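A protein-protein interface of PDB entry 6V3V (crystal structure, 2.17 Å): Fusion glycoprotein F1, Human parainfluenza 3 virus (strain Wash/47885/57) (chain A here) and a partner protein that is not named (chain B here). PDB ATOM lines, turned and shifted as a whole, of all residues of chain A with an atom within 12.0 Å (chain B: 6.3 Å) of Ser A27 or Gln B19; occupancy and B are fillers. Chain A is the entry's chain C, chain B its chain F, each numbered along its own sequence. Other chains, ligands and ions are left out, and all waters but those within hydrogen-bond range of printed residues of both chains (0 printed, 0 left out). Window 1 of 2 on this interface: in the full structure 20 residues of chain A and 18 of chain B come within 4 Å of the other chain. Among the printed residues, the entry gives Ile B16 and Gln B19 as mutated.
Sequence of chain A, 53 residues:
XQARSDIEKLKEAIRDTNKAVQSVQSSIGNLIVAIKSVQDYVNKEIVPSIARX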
ATOM      1  N   ASP A  16      -7.912  14.453  13.091  1.00  0.00           N
ATOM      2  CA  ASP A  16      -9.259  13.893  13.084  1.00  0.00           C
ATOM      3  C   ASP A  16      -9.223  12.384  12.890  1.00  0.00           C
ATOM      4  O   ASP A  16      -9.925  11.639  13.585  1.00  0.00           O
ATOM      5  CB  ASP A  16     -10.087  14.551  11.980  1.00  0.00           C
ATOM      6  CG  ASP A  16     -10.258  16.040  12.189  1.00  0.00           C
ATOM      7  OD1 ASP A  16      -9.939  16.525  13.294  1.00  0.00           O
ATOM      8  OD2 ASP A  16     -10.711  16.726  11.248  1.00  0.00           O
ATOM      9  N   THR A  17      -8.404  11.915  11.945  1.00  0.00           N
ATOM     10  CA  THR A  17      -8.277  10.479  11.718  1.00  0.00           C
ATOM     11  C   THR A  17      -7.786   9.763  12.970  1.00  0.00           C
ATOM     12  O   THR A  17      -8.297   8.694  13.322  1.00  0.00           O
ATOM     13  CB  THR A  17      -7.334  10.222  10.544  1.00  0.00           C
ATOM     14  OG1 THR A  17      -7.813  10.918   9.386  1.00  0.00           O
ATOM     15  CG2 THR A  17      -7.246   8.727  10.242  1.00  0.00           C
ATOM     16  N   ASN A  18      -6.801  10.343  13.661  1.00  0.00           N
ATOM     17  CA  ASN A  18      -6.295   9.727  14.884  1.00  0.00           C
ATOM     18  C   ASN A  18      -7.368   9.674  15.965  1.00  0.00           C
ATOM     19  O   ASN A  18      -7.483   8.674  16.686  1.00  0.00           O
ATOM     20  CB  ASN A  18      -5.060  10.474  15.383  1.00  0.00           C
ATOM     21  CG  ASN A  18      -3.858  10.279  14.481  1.00  0.00           C
ATOM     22  OD1 ASN A  18      -3.762   9.287  13.758  1.00  0.00           O
ATOM     23  ND2 ASN A  18      -2.929  11.226  14.524  1.00  0.00           N
ATOM     24  N   LYS A  19      -8.161  10.744  16.097  1.00  0.00           N
ATOM     25  CA  LYS A  19      -9.263  10.724  17.055  1.00  0.00           C
ATOM     26  C   LYS A  19     -10.268   9.629  16.714  1.00  0.00           C
ATOM     27  O   LYS A  19     -10.769   8.936  17.608  1.00  0.00           O
ATOM     28  CB  LYS A  19      -9.948  12.090  17.115  1.00  0.00           C
ATOM     29  CG  LYS A  19      -9.040  13.243  17.521  1.00  0.00           C
ATOM     30  CD  LYS A  19      -8.406  13.030  18.886  1.00  0.00           C
ATOM     31  CE  LYS A  19      -7.458  14.174  19.228  1.00  0.00           C
ATOM     32  NZ  LYS A  19      -6.881  14.062  20.599  1.00  0.00           N
ATOM     33  N   ALA A  20     -10.571   9.455  15.426  1.00  0.00           N
ATOM     34  CA  ALA A  20     -11.469   8.382  15.013  1.00  0.00           C
ATOM     35  C   ALA A  20     -10.920   7.020  15.416  1.00  0.00           C
ATOM     36  O   ALA A  20     -11.677   6.129  15.822  1.00  0.00           O
ATOM     37  CB  ALA A  20     -11.689   8.442  13.504  1.00  0.00           C
ATOM     38  N   VAL A  21      -9.603   6.839  15.307  1.00  0.00           N
ATOM     39  CA  VAL A  21      -8.989   5.578  15.708  1.00  0.00           C
ATOM     40  C   VAL A  21      -9.054   5.407  17.219  1.00  0.00           C
ATOM     41  O   VAL A  21      -9.328   4.310  17.723  1.00  0.00           O
ATOM     42  CB  VAL A  21      -7.553   5.482  15.163  1.00  0.00           C
ATOM     43  CG1 VAL A  21      -6.879   4.209  15.650  1.00  0.00           C
ATOM     44  CG2 VAL A  21      -7.564   5.538  13.641  1.00  0.00           C
ATOM     45  N   GLN A  22      -8.817   6.487  17.969  1.00  0.00           N
ATOM     46  CA  GLN A  22      -8.913   6.414  19.423  1.00  0.00           C
ATOM     47  C   GLN A  22     -10.318   6.030  19.868  1.00  0.00           C
ATOM     48  O   GLN A  22     -10.488   5.212  20.781  1.00  0.00           O
ATOM     49  CB  GLN A  22      -8.493   7.744  20.048  1.00  0.00           C
ATOM     50  CG  GLN A  22      -7.018   8.070  19.884  1.00  0.00           C
ATOM     51  CD  GLN A  22      -6.616   9.331  20.626  1.00  0.00           C
ATOM     52  OE1 GLN A  22      -7.209  10.392  20.437  1.00  0.00           O
ATOM     53  NE2 GLN A  22      -5.606   9.218  21.482  1.00  0.00           N
ATOM     54  N   SER A  23     -11.340   6.609  19.235  1.00  0.00           N
ATOM     55  CA  SER A  23     -12.715   6.239  19.554  1.00  0.00           C
ATOM     56  C   SER A  23     -12.987   4.773  19.235  1.00  0.00           C
ATOM     57  O   SER A  23     -13.757   4.113  19.944  1.00  0.00           O
ATOM     58  CB  SER A  23     -13.685   7.144  18.797  1.00  0.00           C
ATOM     59  OG  SER A  23     -15.027   6.832  19.120  1.00  0.00           O
ATOM     60  N   VAL A  24     -12.365   4.247  18.177  1.00  0.00           N
ATOM     61  CA  VAL A  24     -12.494   2.828  17.863  1.00  0.00           C
ATOM     62  C   VAL A  24     -11.793   1.980  18.917  1.00  0.00           C
ATOM     63  O   VAL A  24     -12.270   0.899  19.285  1.00  0.00           O
ATOM     64  CB  VAL A  24     -11.968   2.552  16.442  1.00  0.00           C
ATOM     65  CG1 VAL A  24     -11.669   1.076  16.248  1.00  0.00           C
ATOM     66  CG2 VAL A  24     -12.974   3.029  15.406  1.00  0.00           C
ATOM     67  N   GLN A  25     -10.659   2.463  19.433  1.00  0.00           N
ATOM     68  CA  GLN A  25      -9.922   1.710  20.441  1.00  0.00           C
ATOM     69  C   GLN A  25     -10.726   1.568  21.728  1.00  0.00           C
ATOM     70  O   GLN A  25     -10.682   0.521  22.384  1.00  0.00           O
ATOM     71  CB  GLN A  25      -8.572   2.378  20.704  1.00  0.00           C
ATOM     72  CG  GLN A  25      -7.640   2.336  19.502  1.00  0.00           C
ATOM     73  CD  GLN A  25      -6.465   3.290  19.626  1.00  0.00           C
ATOM     74  OE1 GLN A  25      -6.534   4.293  20.337  1.00  0.00           O
ATOM     75  NE2 GLN A  25      -5.377   2.980  18.929  1.00  0.00           N
ATOM     76  N   SER A  26     -11.474   2.609  22.100  1.00  0.00           N
ATOM     77  CA  SER A  26     -12.338   2.509  23.270  1.00  0.00           C
ATOM     78  C   SER A  26     -13.455   1.497  23.046  1.00  0.00           C
ATOM     79  O   SER A  26     -13.780   0.713  23.946  1.00  0.00           O
ATOM     80  CB  SER A  26     -12.919   3.880  23.611  1.00  0.00           C
ATOM     81  OG  SER A  26     -11.891   4.815  23.884  1.00  0.00           O
ATOM     82  N   SER A  27     -14.051   1.496  21.850  1.00  0.00           N
ATOM     83  CA  SER A  27     -15.138   0.564  21.563  1.00  0.00           C
ATOM     84  C   SER A  27     -14.659  -0.881  21.620  1.00  0.00           C
ATOM     85  O   SER A  27     -15.386  -1.764  22.091  1.00  0.00           O
ATOM     86  CB  SER A  27     -15.762   0.882  20.204  1.00  0.00           C
ATOM     87  OG  SER A  27     -14.849   0.627  19.153  1.00  0.00           O
ATOM     88  N   ILE A  28     -13.439  -1.145  21.146  1.00  0.00           N
ATOM     89  CA  ILE A  28     -12.870  -2.485  21.281  1.00  0.00           C
ATOM     90  C   ILE A  28     -12.670  -2.826  22.750  1.00  0.00           C
ATOM     91  O   ILE A  28     -12.917  -3.960  23.180  1.00  0.00           O
ATOM     92  CB  ILE A  28     -11.561  -2.606  20.479  1.00  0.00           C
ATOM     93  CG1 ILE A  28     -11.811  -2.324  18.997  1.00  0.00           C
ATOM     94  CG2 ILE A  28     -10.950  -3.989  20.663  1.00  0.00           C
ATOM     95  CD1 ILE A  28     -10.546  -2.244  18.181  1.00  0.00           C
ATOM     96  N   GLY A  29     -12.224  -1.847  23.542  1.00  0.00           N
ATOM     97  CA  GLY A  29     -12.045  -2.079  24.966  1.00  0.00           C
ATOM     98  C   GLY A  29     -13.325  -2.520  25.648  1.00  0.00           C
ATOM     99  O   GLY A  29     -13.315  -3.437  26.473  1.00  0.00           O
ATOM    100  N   ASN A  30     -14.446  -1.884  25.306  1.00  0.00           N
ATOM    101  CA  ASN A  30     -15.718  -2.291  25.891  1.00  0.00           C
ATOM    102  C   ASN A  30     -16.218  -3.607  25.301  1.00  0.00           C
ATOM    103  O   ASN A  30     -16.970  -4.328  25.966  1.00  0.00           O
ATOM    104  CB  ASN A  30     -16.756  -1.182  25.737  1.00  0.00           C
ATOM    105  CG  ASN A  30     -16.440   0.032  26.583  1.00  0.00           C
ATOM    106  OD1 ASN A  30     -16.041  -0.090  27.741  1.00  0.00           O
ATOM    107  ND2 ASN A  30     -16.604   1.216  26.003  1.00  0.00           N
ATOM    108  N   LEU A  31     -15.822  -3.935  24.066  1.00  0.00           N
ATOM    109  CA  LEU A  31     -16.154  -5.242  23.504  1.00  0.00           C
ATOM    110  C   LEU A  31     -15.493  -6.363  24.297  1.00  0.00           C
ATOM    111  O   LEU A  31     -16.095  -7.421  24.514  1.00  0.00           O
ATOM    112  CB  LEU A  31     -15.741  -5.304  22.034  1.00  0.00           C
ATOM    113  CG  LEU A  31     -16.627  -4.593  21.011  1.00  0.00           C
ATOM    114  CD1 LEU A  31     -15.903  -4.464  19.682  1.00  0.00           C
ATOM    115  CD2 LEU A  31     -17.939  -5.343  20.837  1.00  0.00           C
ATOM    116  N   ILE A  32     -14.246  -6.153  24.724  1.00  0.00           N
ATOM    117  CA  ILE A  32     -13.594  -7.102  25.623  1.00  0.00           C
ATOM    118  C   ILE A  32     -14.428  -7.293  26.883  1.00  0.00           C
ATOM    119  O   ILE A  32     -14.645  -8.419  27.345  1.00  0.00           O
ATOM    120  CB  ILE A  32     -12.168  -6.627  25.952  1.00  0.00           C
ATOM    121  CG1 ILE A  32     -11.314  -6.563  24.684  1.00  0.00           C
ATOM    122  CG2 ILE A  32     -11.529  -7.526  27.006  1.00  0.00           C
ATOM    123  CD1 ILE A  32      -9.944  -5.944  24.911  1.00  0.00           C
ATOM    124  N   VAL A  33     -14.919  -6.188  27.450  1.00  0.00           N
ATOM    125  CA  VAL A  33     -15.753  -6.264  28.647  1.00  0.00           C
ATOM    126  C   VAL A  33     -17.050  -7.009  28.353  1.00  0.00           C
ATOM    127  O   VAL A  33     -17.517  -7.817  29.165  1.00  0.00           O
ATOM    128  CB  VAL A  33     -16.010  -4.851  29.204  1.00  0.00           C
ATOM    129  CG1 VAL A  33     -16.849  -4.923  30.469  1.00  0.00           C
ATOM    130  CG2 VAL A  33     -14.692  -4.137  29.469  1.00  0.00           C
ATOM    131  N   ALA A  34     -17.654  -6.746  27.191  1.00  0.00           N
ATOM    132  CA  ALA A  34     -18.894  -7.424  26.830  1.00  0.00           C
ATOM    133  C   ALA A  34     -18.698  -8.933  26.782  1.00  0.00           C
ATOM    134  O   ALA A  34     -19.542  -9.694  27.269  1.00  0.00           O
ATOM    135  CB  ALA A  34     -19.400  -6.903  25.485  1.00  0.00           C
ATOM    136  N   ILE A  35     -17.581  -9.383  26.208  1.00  0.00           N
ATOM    137  CA  ILE A  35     -17.304 -10.813  26.140  1.00  0.00           C
ATOM    138  C   ILE A  35     -17.019 -11.375  27.529  1.00  0.00           C
ATOM    139  O   ILE A  35     -17.428 -12.496  27.853  1.00  0.00           O
ATOM    140  CB  ILE A  35     -16.169 -11.088  25.138  1.00  0.00           C
ATOM    141  CG1 ILE A  35     -16.581 -10.618  23.740  1.00  0.00           C
ATOM    142  CG2 ILE A  35     -15.806 -12.562  25.122  1.00  0.00           C
ATOM    143  CD1 ILE A  35     -15.532 -10.864  22.681  1.00  0.00           C
ATOM    144  N   LYS A  36     -16.325 -10.606  28.375  1.00  0.00           N
ATOM    145  CA  LYS A  36     -16.073 -11.052  29.744  1.00  0.00           C
ATOM    146  C   LYS A  36     -17.377 -11.243  30.512  1.00  0.00           C
ATOM    147  O   LYS A  36     -17.501 -12.176  31.315  1.00  0.00           O
ATOM    148  CB  LYS A  36     -15.170 -10.056  30.471  1.00  0.00           C
ATOM    149  CG  LYS A  36     -13.745 -10.535  30.699  1.00  0.00           C
ATOM    150  CD  LYS A  36     -12.894 -10.408  29.445  1.00  0.00           C
ATOM    151  CE  LYS A  36     -11.419 -10.639  29.755  1.00  0.00           C
ATOM    152  NZ  LYS A  36     -10.869  -9.611  30.681  1.00  0.00           N
ATOM    153  N   SER A  37     -18.356 -10.361  30.287  1.00  0.00           N
ATOM    154  CA  SER A  37     -19.656 -10.518  30.930  1.00  0.00           C
ATOM    155  C   SER A  37     -20.313 -11.833  30.530  1.00  0.00           C
ATOM    156  O   SER A  37     -20.941 -12.500  31.361  1.00  0.00           O
ATOM    157  CB  SER A  37     -20.566  -9.342  30.572  1.00  0.00           C
ATOM    158  OG  SER A  37     -19.992  -8.112  30.979  1.00  0.00           O
ATOM    159  N   ASN B  14     -23.915  -0.220  25.122  1.00  0.00           N
ATOM    160  CA  ASN B  14     -24.380   1.112  24.739  1.00  0.00           C
ATOM    161  C   ASN B  14     -23.213   2.043  24.438  1.00  0.00           C
ATOM    162  O   ASN B  14     -23.260   2.809  23.469  1.00  0.00           O
ATOM    163  CB  ASN B  14     -25.271   1.699  25.836  1.00  0.00           C
ATOM    164  CG  ASN B  14     -25.871   3.036  25.446  1.00  0.00           C
ATOM    165  OD1 ASN B  14     -25.308   4.094  25.734  1.00  0.00           O
ATOM    166  ND2 ASN B  14     -27.022   2.995  24.787  1.00  0.00           N
ATOM    167  N   LYS B  15     -22.159   1.989  25.257  1.00  0.00           N
ATOM    168  CA  LYS B  15     -20.980   2.815  25.009  1.00  0.00           C
ATOM    169  C   LYS B  15     -20.375   2.521  23.641  1.00  0.00           C
ATOM    170  O   LYS B  15     -19.998   3.447  22.912  1.00  0.00           O
ATOM    171  CB  LYS B  15     -19.939   2.596  26.107  1.00  0.00           C
ATOM    172  CG  LYS B  15     -20.378   3.024  27.494  1.00  0.00           C
ATOM    173  CD  LYS B  15     -19.245   2.851  28.490  1.00  0.00           C
ATOM    174  CE  LYS B  15     -19.693   3.176  29.904  1.00  0.00           C
ATOM    175  NZ  LYS B  15     -20.226   4.560  30.010  1.00  0.00           N
ATOM    176  N   ILE B  16     -20.275   1.238  23.280  1.00  0.00           N
ATOM    177  CA  ILE B  16     -19.696   0.860  21.992  1.00  0.00           C
ATOM    178  C   ILE B  16     -20.478   1.493  20.850  1.00  0.00           C
ATOM    179  O   ILE B  16     -19.903   2.104  19.942  1.00  0.00           O
ATOM    180  CB  ILE B  16     -19.631  -0.671  21.857  1.00  0.00           C
ATOM    181  CG1 ILE B  16     -18.931  -1.279  23.068  1.00  0.00           C
ATOM    182  CG2 ILE B  16     -18.909  -1.053  20.582  1.00  0.00           C
ATOM    183  CD1 ILE B  16     -19.035  -2.783  23.147  1.00  0.00           C
ATOM    184  N   LYS B  17     -21.805   1.356  20.880  1.00  0.00           N
ATOM    185  CA  LYS B  17     -22.638   1.975  19.855  1.00  0.00           C
ATOM    186  C   LYS B  17     -22.441   3.486  19.824  1.00  0.00           C
ATOM    187  O   LYS B  17     -22.427   4.096  18.748  1.00  0.00           O
ATOM    188  CB  LYS B  17     -24.105   1.618  20.093  1.00  0.00           C
ATOM    189  CG  LYS B  17     -25.063   2.171  19.049  1.00  0.00           C
ATOM    190  CD  LYS B  17     -24.699   1.700  17.648  1.00  0.00           C
ATOM    191  CE  LYS B  17     -25.689   2.225  16.618  1.00  0.00           C
ATOM    192  NZ  LYS B  17     -25.287   1.877  15.226  1.00  0.00           N
ATOM    193  N   SER B  18     -22.276   4.109  20.996  1.00  0.00           N
ATOM    194  CA  SER B  18     -22.030   5.547  21.042  1.00  0.00           C
ATOM    195  C   SER B  18     -20.600   5.877  20.639  1.00  0.00           C
ATOM    196  O   SER B  18     -20.368   6.823  19.877  1.00  0.00           O
ATOM    197  CB  SER B  18     -22.345   6.097  22.433  1.00  0.00           C
ATOM    198  OG  SER B  18     -23.737   6.052  22.694  1.00  0.00           O
ATOM    199  N   GLN B  19     -19.625   5.112  21.141  1.00  0.00           N
ATOM    200  CA  GLN B  19     -18.239   5.328  20.739  1.00  0.00           C
ATOM    201  C   GLN B  19     -18.042   5.057  19.254  1.00  0.00           C
ATOM    202  O   GLN B  19     -17.127   5.614  18.637  1.00  0.00           O
ATOM    203  CB  GLN B  19     -17.302   4.457  21.576  1.00  0.00           C
ATOM    204  CG  GLN B  19     -17.146   4.926  23.014  1.00  0.00           C
ATOM    205  CD  GLN B  19     -16.519   3.873  23.906  1.00  0.00           C
ATOM    206  OE1 GLN B  19     -16.552   2.684  23.595  1.00  0.00           O
ATOM    207  NE2 GLN B  19     -15.944   4.306  25.023  1.00  0.00           N
ATOM    208  N   LEU B  20     -18.888   4.209  18.666  1.00  0.00           N
ATOM    209  CA  LEU B  20     -18.828   3.984  17.227  1.00  0.00           C
ATOM    210  C   LEU B  20     -19.312   5.207  16.462  1.00  0.00           C
ATOM    211  O   LEU B  20     -18.679   5.625  15.485  1.00  0.00           O
ATOM    212  CB  LEU B  20     -19.661   2.757  16.856  1.00  0.00           C
ATOM    213  CG  LEU B  20     -19.609   2.328  15.391  1.00  0.00           C
ATOM    214  CD1 LEU B  20     -18.187   1.959  15.011  1.00  0.00           C
ATOM    215  CD2 LEU B  20     -20.560   1.168  15.138  1.00  0.00           C
ATOM    216  N   GLU B  21     -20.430   5.797  16.894  1.00  0.00           N
ATOM    217  CA  GLU B  21     -20.978   6.951  16.187  1.00  0.00           C
ATOM    218  C   GLU B  21     -20.038   8.146  16.257  1.00  0.00           C
ATOM    219  O   GLU B  21     -19.901   8.891  15.280  1.00  0.00           O
ATOM    220  CB  GLU B  21     -22.359   7.308  16.737  1.00  0.00           C
ATOM    221  CG  GLU B  21     -23.477   6.467  16.153  1.00  0.00           C
ATOM    222  CD  GLU B  21     -23.578   6.607  14.645  1.00  0.00           C
ATOM    223  OE1 GLU B  21     -23.368   7.728  14.134  1.00  0.00           O
ATOM    224  OE2 GLU B  21     -23.860   5.594  13.971  1.00  0.00           O
ATOM    225  N   GLU B  22     -19.384   8.349  17.402  1.00  0.00           N
ATOM    226  CA  GLU B  22     -18.418   9.436  17.507  1.00  0.00           C
ATOM    227  C   GLU B  22     -17.229   9.221  16.578  1.00  0.00           C
ATOM    228  O   GLU B  22     -16.686  10.190  16.037  1.00  0.00           O
ATOM    229  CB  GLU B  22     -17.961   9.602  18.957  1.00  0.00           C
ATOM    230  CG  GLU B  22     -19.065  10.058  19.898  1.00  0.00           C
ATOM    231  CD  GLU B  22     -18.579  10.253  21.320  1.00  0.00           C
ATOM    232  OE1 GLU B  22     -17.411   9.906  21.600  1.00  0.00           O
ATOM    233  OE2 GLU B  22     -19.363  10.752  22.155  1.00  0.00           O
ATOM    234  N   SER B  23     -16.821   7.966  16.372  1.00  0.00           N
ATOM    235  CA  SER B  23     -15.738   7.695  15.435  1.00  0.00           C
ATOM    236  C   SER B  23     -16.156   7.983  14.000  1.00  0.00           C
ATOM    237  O   SER B  23     -15.331   8.424  13.191  1.00  0.00           O
ATOM    238  CB  SER B  23     -15.267   6.248  15.577  1.00  0.00           C
ATOM    239  OG  SER B  23     -14.189   5.973  14.699  1.00  0.00           O
ATOM    240  N   LYS B  24     -17.423   7.735  13.663  1.00  0.00           N
ATOM    241  CA  LYS B  24     -17.903   8.042  12.321  1.00  0.00           C
ATOM    242  C   LYS B  24     -17.816   9.535  12.037  1.00  0.00           C
ATOM    243  O   LYS B  24     -17.434   9.944  10.934  1.00  0.00           O
ATOM    244  CB  LYS B  24     -19.341   7.547  12.155  1.00  0.00           C
ATOM    245  CG  LYS B  24     -19.508   6.041  12.299  1.00  0.00           C
ATOM    246  CD  LYS B  24     -20.968   5.631  12.164  1.00  0.00           C
ATOM    247  CE  LYS B  24     -21.135   4.124  12.313  1.00  0.00           C
ATOM    248  NZ  LYS B  24     -22.563   3.710  12.200  1.00  0.00           N
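The backbone NH (N) of Ser A27 lies close to the side-chain amide oxygen (OE1) of Gln B19 (3.3 Å). The side-chain amide oxygen of Gln B19 sits close to the backbone carbonyl oxygen of Ser A26, at 3.4 Å. OG of Ser A23 is in hydrogen-bond range of O of Gln B19. OG of Ser A23 lies within hydrogen-bond range of N of Ser B23. The backbone carbonyl oxygen (O) of Ala A20 sits at hydrogen-bond distance from the side-chain hydroxyl (OG) of Ser B23 (2.8 Å). The side-chain amide nitrogen (ND2) of Asn A30 sits at hydrogen-bond distance from the side-chain amide oxygen (OE1) of Gln B19 (2.8 Å).
O of Val A24 sits at hydrogen-bond distance from OG of Ser A27 (2.6 Å). The backbone carbonyl oxygen (O) of Gln A22 sits at hydrogen-bond distance from the side-chain hydroxyl (OG) of Ser A26.
Ser B23 touches Val A24 (OG to CG2, 3.3 Å). Ile B16 touches Ser A27. ND2 of Asn A30 touches CB of Lys B15, at 3.6 Å. Asn A30 touches Ile B16. Leu A31 touches Ile B16.
Of the printed residues of chain B, Ala A20 touches Ser B23. Printed residues of chain B within 4 Å of Val A24: Ser B23. Of the printed residues of chain B, Ser A26 touches Gln B19. Ser A27 touches two residues of chain B. Printed residues of chain A within 4 Å of Ile B16: Ser A27 (3.7 Å), Asn A30 (3.4 Å) and Leu A31 (3.5 Å). Gln B19 touches four residues of chain A. No residue of chain A comes within 4 Å of Leu B20. No residue of chain A comes within 4 Å of Glu B22. Printed residues of chain A within 4 Å of Ser B23: Ala A20, Ser A23 and Val A24. The nearest residue of chain A that does not touch Gln B19 is Val A24 (5.0 Å). The nearest printed residue of chain B that does not touch Ser A26 is Ile B16 (5.6 Å).
Of the 11 printed residues of chain B, 4 touch a printed residue of chain A. Along chain B the printed residues that touch a printed residue of chain A span positions 15 to 23. Of the 22 printed residues of chain A, 7 touch a printed residue of chain B. Hydrophobic or aromatic side chains of chain A within 4 Å of the printed part of chain B: Ala A20, Val A24 and Leu A31. Among the printed residues, no Asp or Glu carboxylate lies within 4 Å of a Lys or Arg side-chain nitrogen of the other chain.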
